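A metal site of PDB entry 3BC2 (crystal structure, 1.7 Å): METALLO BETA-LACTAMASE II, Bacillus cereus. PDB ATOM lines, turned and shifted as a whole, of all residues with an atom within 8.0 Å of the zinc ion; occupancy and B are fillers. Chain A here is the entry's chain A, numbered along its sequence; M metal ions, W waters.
A ring nitrogen (NE2) of His 88 lies within hydrogen-bond range of the side-chain carboxylate (OD2) of Asp 183.
The side-chain amide oxygen (OD1) of Asn 153 sits at hydrogen-bond distance from the backbone NH (N) of His 149 (2.8 Å).
OD1 of CSD 168 lies within salt-bridge range of NH2 of Arg 91 (2.9 Å).
CSD 168 touches the zinc ion (OD2 to ZN, 3.7 Å).
Four residues have an atom within 4 Å of the zinc ion: His 86, His 88, His 149 and CSD 168.
ND1 of His 88 is bound to the zinc ion.
A ring nitrogen (NE2) of His 149 is bound to the zinc ion (2.1 Å).
The zinc ion is bound by NE2 of His 86, 2.3 Å away.
The zinc ion is bound by water W1 (2.5 Å).
Slightly farther from the zinc ion lies water W2 (2.8 Å).
Water W1 lies within hydrogen-bond range of OD2 of CSD 168 (2.8 Å) and OD1 of Asp 90 (2.8 Å).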
ATOM      1  N   THR A  85     -25.239  32.819 -25.733  1.00  0.00           N
ATOM      2  CA  THR A  85     -23.769  32.896 -25.822  1.00  0.00           C
ATOM      3  C   THR A  85     -23.041  31.934 -26.782  1.00  0.00           C
ATOM      4  O   THR A  85     -21.900  32.184 -27.147  1.00  0.00           O
ATOM      5  CB  THR A  85     -23.102  32.907 -24.434  1.00  0.00           C
ATOM      6  OG1 THR A  85     -23.476  31.732 -23.703  1.00  0.00           O
ATOM      7  CG2 THR A  85     -23.519  34.156 -23.663  1.00  0.00           C
ATOM      8  N   HIS A  86     -23.702  30.833 -27.124  1.00  0.00           N
ATOM      9  CA  HIS A  86     -23.205  29.871 -28.116  1.00  0.00           C
ATOM     10  C   HIS A  86     -24.300  28.857 -28.472  1.00  0.00           C
ATOM     11  O   HIS A  86     -25.305  28.721 -27.752  1.00  0.00           O
ATOM     12  CB  HIS A  86     -21.836  29.233 -27.780  1.00  0.00           C
ATOM     13  CG  HIS A  86     -21.867  28.207 -26.694  1.00  0.00           C
ATOM     14  ND1 HIS A  86     -21.700  28.534 -25.369  1.00  0.00           N
ATOM     15  CD2 HIS A  86     -21.983  26.862 -26.741  1.00  0.00           C
ATOM     16  CE1 HIS A  86     -21.715  27.424 -24.646  1.00  0.00           C
ATOM     17  NE2 HIS A  86     -21.875  26.394 -25.454  1.00  0.00           N
ATOM     18  N   ALA A  87     -24.125  28.176 -29.602  1.00  0.00           N
ATOM     19  CA  ALA A  87     -25.132  27.245 -30.101  1.00  0.00           C
ATOM     20  C   ALA A  87     -25.350  25.874 -29.488  1.00  0.00           C
ATOM     21  O   ALA A  87     -26.238  25.145 -29.948  1.00  0.00           O
ATOM     22  CB  ALA A  87     -25.002  27.122 -31.617  1.00  0.00           C
ATOM     23  N   HIS A  88     -24.568  25.482 -28.483  1.00  0.00           N
ATOM     24  CA  HIS A  88     -24.750  24.173 -27.876  1.00  0.00           C
ATOM     25  C   HIS A  88     -26.139  23.999 -27.225  1.00  0.00           C
ATOM     26  O   HIS A  88     -26.733  24.966 -26.741  1.00  0.00           O
ATOM     27  CB  HIS A  88     -23.659  23.882 -26.844  1.00  0.00           C
ATOM     28  CG  HIS A  88     -22.396  23.317 -27.423  1.00  0.00           C
ATOM     29  ND1 HIS A  88     -21.180  23.405 -26.779  1.00  0.00           N
ATOM     30  CD2 HIS A  88     -22.169  22.646 -28.578  1.00  0.00           C
ATOM     31  CE1 HIS A  88     -20.256  22.821 -27.527  1.00  0.00           C
ATOM     32  NE2 HIS A  88     -20.827  22.357 -28.622  1.00  0.00           N
ATOM     33  N   ALA A  89     -26.618  22.761 -27.209  1.00  0.00           N
ATOM     34  CA  ALA A  89     -27.907  22.386 -26.637  1.00  0.00           C
ATOM     35  C   ALA A  89     -28.222  23.009 -25.272  1.00  0.00           C
ATOM     36  O   ALA A  89     -29.364  23.385 -25.015  1.00  0.00           O
ATOM     37  CB  ALA A  89     -28.021  20.871 -26.548  1.00  0.00           C
ATOM     38  N   ASP A  90     -27.222  23.118 -24.401  1.00  0.00           N
ATOM     39  CA  ASP A  90     -27.431  23.687 -23.065  1.00  0.00           C
ATOM     40  C   ASP A  90     -27.767  25.182 -23.080  1.00  0.00           C
ATOM     41  O   ASP A  90     -28.344  25.703 -22.120  1.00  0.00           O
ATOM     42  CB  ASP A  90     -26.229  23.399 -22.153  1.00  0.00           C
ATOM     43  CG  ASP A  90     -25.046  24.323 -22.404  1.00  0.00           C
ATOM     44  OD1 ASP A  90     -24.736  24.620 -23.580  1.00  0.00           O
ATOM     45  OD2 ASP A  90     -24.397  24.751 -21.413  1.00  0.00           O
ATOM     46  N   ARG A  91     -27.403  25.853 -24.165  1.00  0.00           N
ATOM     47  CA  ARG A  91     -27.669  27.285 -24.324  1.00  0.00           C
ATOM     48  C   ARG A  91     -28.825  27.547 -25.291  1.00  0.00           C
ATOM     49  O   ARG A  91     -29.645  28.430 -25.052  1.00  0.00           O
ATOM     50  CB  ARG A  91     -26.420  28.010 -24.827  1.00  0.00           C
ATOM     51  CG  ARG A  91     -25.205  27.853 -23.934  1.00  0.00           C
ATOM     52  CD  ARG A  91     -25.502  28.328 -22.520  1.00  0.00           C
ATOM     53  NE  ARG A  91     -24.384  28.114 -21.602  1.00  0.00           N
ATOM     54  CZ  ARG A  91     -24.430  28.329 -20.295  1.00  0.00           C
ATOM     55  NH1 ARG A  91     -25.555  28.757 -19.725  1.00  0.00           N
ATOM     56  NH2 ARG A  91     -23.356  28.142 -19.545  1.00  0.00           N
ATOM     57  N   HIS A 149     -14.166  27.594 -26.406  1.00  0.00           N
ATOM     58  CA  HIS A 149     -15.025  26.456 -26.052  1.00  0.00           C
ATOM     59  C   HIS A 149     -15.726  25.923 -27.305  1.00  0.00           C
ATOM     60  O   HIS A 149     -15.947  24.714 -27.448  1.00  0.00           O
ATOM     61  CB  HIS A 149     -16.065  26.907 -25.024  1.00  0.00           C
ATOM     62  CG  HIS A 149     -17.134  25.902 -24.759  1.00  0.00           C
ATOM     63  ND1 HIS A 149     -16.895  24.724 -24.091  1.00  0.00           N
ATOM     64  CD2 HIS A 149     -18.450  25.888 -25.079  1.00  0.00           C
ATOM     65  CE1 HIS A 149     -18.012  24.025 -24.009  1.00  0.00           C
ATOM     66  NE2 HIS A 149     -18.971  24.716 -24.610  1.00  0.00           N
ATOM     67  N   THR A 150     -16.127  26.850 -28.180  1.00  0.00           N
ATOM     68  CA  THR A 150     -16.762  26.547 -29.457  1.00  0.00           C
ATOM     69  C   THR A 150     -16.244  27.587 -30.411  1.00  0.00           C
ATOM     70  O   THR A 150     -15.512  28.489 -30.012  1.00  0.00           O
ATOM     71  CB  THR A 150     -18.315  26.662 -29.420  1.00  0.00           C
ATOM     72  OG1 THR A 150     -18.711  27.894 -28.814  1.00  0.00           O
ATOM     73  CG2 THR A 150     -18.929  25.520 -28.674  1.00  0.00           C
ATOM     74  N   ASP A 152     -18.103  29.763 -31.977  1.00  0.00           N
ATOM     75  CA  ASP A 152     -18.963  30.942 -31.846  1.00  0.00           C
ATOM     76  C   ASP A 152     -19.136  31.630 -30.495  1.00  0.00           C
ATOM     77  O   ASP A 152     -19.805  32.665 -30.431  1.00  0.00           O
ATOM     78  CB  ASP A 152     -20.358  30.572 -32.378  1.00  0.00           C
ATOM     79  CG  ASP A 152     -21.056  29.547 -31.515  1.00  0.00           C
ATOM     80  OD1 ASP A 152     -20.428  28.538 -31.114  1.00  0.00           O
ATOM     81  OD2 ASP A 152     -22.254  29.720 -31.238  1.00  0.00           O
ATOM     82  N   ASN A 153     -18.560  31.076 -29.422  1.00  0.00           N
ATOM     83  CA  ASN A 153     -18.734  31.675 -28.091  1.00  0.00           C
ATOM     84  C   ASN A 153     -18.499  33.163 -27.926  1.00  0.00           C
ATOM     85  O   ASN A 153     -17.532  33.726 -28.446  1.00  0.00           O
ATOM     86  CB  ASN A 153     -18.009  30.868 -26.997  1.00  0.00           C
ATOM     87  CG  ASN A 153     -16.498  30.758 -27.203  1.00  0.00           C
ATOM     88  OD1 ASN A 153     -15.886  29.809 -26.740  1.00  0.00           O
ATOM     89  ND2 ASN A 153     -15.894  31.748 -27.853  1.00  0.00           N
ATOM     90  N   GLY A 167     -19.635  32.774 -19.987  1.00  0.00           N
ATOM     91  CA  GLY A 167     -20.176  31.597 -20.631  1.00  0.00           C
ATOM     92  C   GLY A 167     -19.181  30.467 -20.473  1.00  0.00           C
ATOM     93  O   GLY A 167     -18.367  30.470 -19.544  1.00  0.00           O
ATOM     94  N   CSD A 168     -19.202  29.509 -21.381  1.00  0.00           N
ATOM     95  CA  CSD A 168     -18.284  28.393 -21.297  1.00  0.00           C
ATOM     96  CB  CSD A 168     -18.883  27.167 -21.968  1.00  0.00           C
ATOM     97  SG  CSD A 168     -20.245  26.524 -21.001  1.00  0.00           S
ATOM     98  C   CSD A 168     -16.848  28.660 -21.761  1.00  0.00           C
ATOM     99  O   CSD A 168     -16.024  27.758 -21.747  1.00  0.00           O
ATOM    100  OD1 CSD A 168     -21.335  27.457 -21.477  1.00  0.00           O
ATOM    101  OD2 CSD A 168     -20.625  25.182 -21.531  1.00  0.00           O
ATOM    102  N   LEU A 169     -16.564  29.896 -22.161  1.00  0.00           N
ATOM    103  CA  LEU A 169     -15.216  30.303 -22.562  1.00  0.00           C
ATOM    104  C   LEU A 169     -14.344  30.398 -21.319  1.00  0.00           C
ATOM    105  O   LEU A 169     -13.127  30.332 -21.384  1.00  0.00           O
ATOM    106  CB  LEU A 169     -15.225  31.683 -23.211  1.00  0.00           C
ATOM    107  CG  LEU A 169     -13.862  32.262 -23.589  1.00  0.00           C
ATOM    108  CD1 LEU A 169     -13.354  31.580 -24.846  1.00  0.00           C
ATOM    109  CD2 LEU A 169     -13.962  33.750 -23.829  1.00  0.00           C
ATOM    110  N   ASN A 180     -16.066  19.230 -22.235  1.00  0.00           N
ATOM    111  CA  ASN A 180     -16.205  18.654 -23.570  1.00  0.00           C
ATOM    112  C   ASN A 180     -15.522  19.561 -24.579  1.00  0.00           C
ATOM    113  O   ASN A 180     -15.986  20.679 -24.838  1.00  0.00           O
ATOM    114  CB  ASN A 180     -17.673  18.440 -23.924  1.00  0.00           C
ATOM    115  CG  ASN A 180     -18.288  17.267 -23.177  1.00  0.00           C
ATOM    116  OD1 ASN A 180     -18.974  17.438 -22.171  1.00  0.00           O
ATOM    117  ND2 ASN A 180     -18.017  16.049 -23.656  1.00  0.00           N
ATOM    118  N   ASP A 183     -16.033  20.362 -29.775  1.00  0.00           N
ATOM    119  CA  ASP A 183     -16.207  21.457 -30.706  1.00  0.00           C
ATOM    120  C   ASP A 183     -15.312  22.648 -30.356  1.00  0.00           C
ATOM    121  O   ASP A 183     -15.491  23.746 -30.874  1.00  0.00           O
ATOM    122  CB  ASP A 183     -17.674  21.895 -30.737  1.00  0.00           C
ATOM    123  CG  ASP A 183     -18.633  20.737 -31.024  1.00  0.00           C
ATOM    124  OD1 ASP A 183     -18.298  19.828 -31.805  1.00  0.00           O
ATOM    125  OD2 ASP A 183     -19.749  20.750 -30.474  1.00  0.00           O
ATOM    126  N   HIS A 210     -20.389  27.604 -15.972  1.00  0.00           N
ATOM    127  CA  HIS A 210     -20.730  26.639 -14.916  1.00  0.00           C
ATOM    128  C   HIS A 210     -19.858  26.985 -13.709  1.00  0.00           C
ATOM    129  O   HIS A 210     -18.750  27.502 -13.863  1.00  0.00           O
ATOM    130  CB  HIS A 210     -20.424  25.208 -15.376  1.00  0.00           C
ATOM    131  CG  HIS A 210     -21.282  24.721 -16.498  1.00  0.00           C
ATOM    132  ND1 HIS A 210     -22.318  23.829 -16.318  1.00  0.00           N
ATOM    133  CD2 HIS A 210     -21.240  24.987 -17.833  1.00  0.00           C
ATOM    134  CE1 HIS A 210     -22.883  23.565 -17.485  1.00  0.00           C
ATOM    135  NE2 HIS A 210     -22.242  24.264 -18.416  1.00  0.00           N
HETATM  136 ZN    ZN M   1     -20.991  24.339 -25.096  1.00  0.00          ZN
HETATM  137  O   HOH W   1     -22.191  23.504 -23.060  1.00  0.00           O
HETATM  138  O   HOH W   2     -20.167  21.746 -24.267  1.00  0.00           O
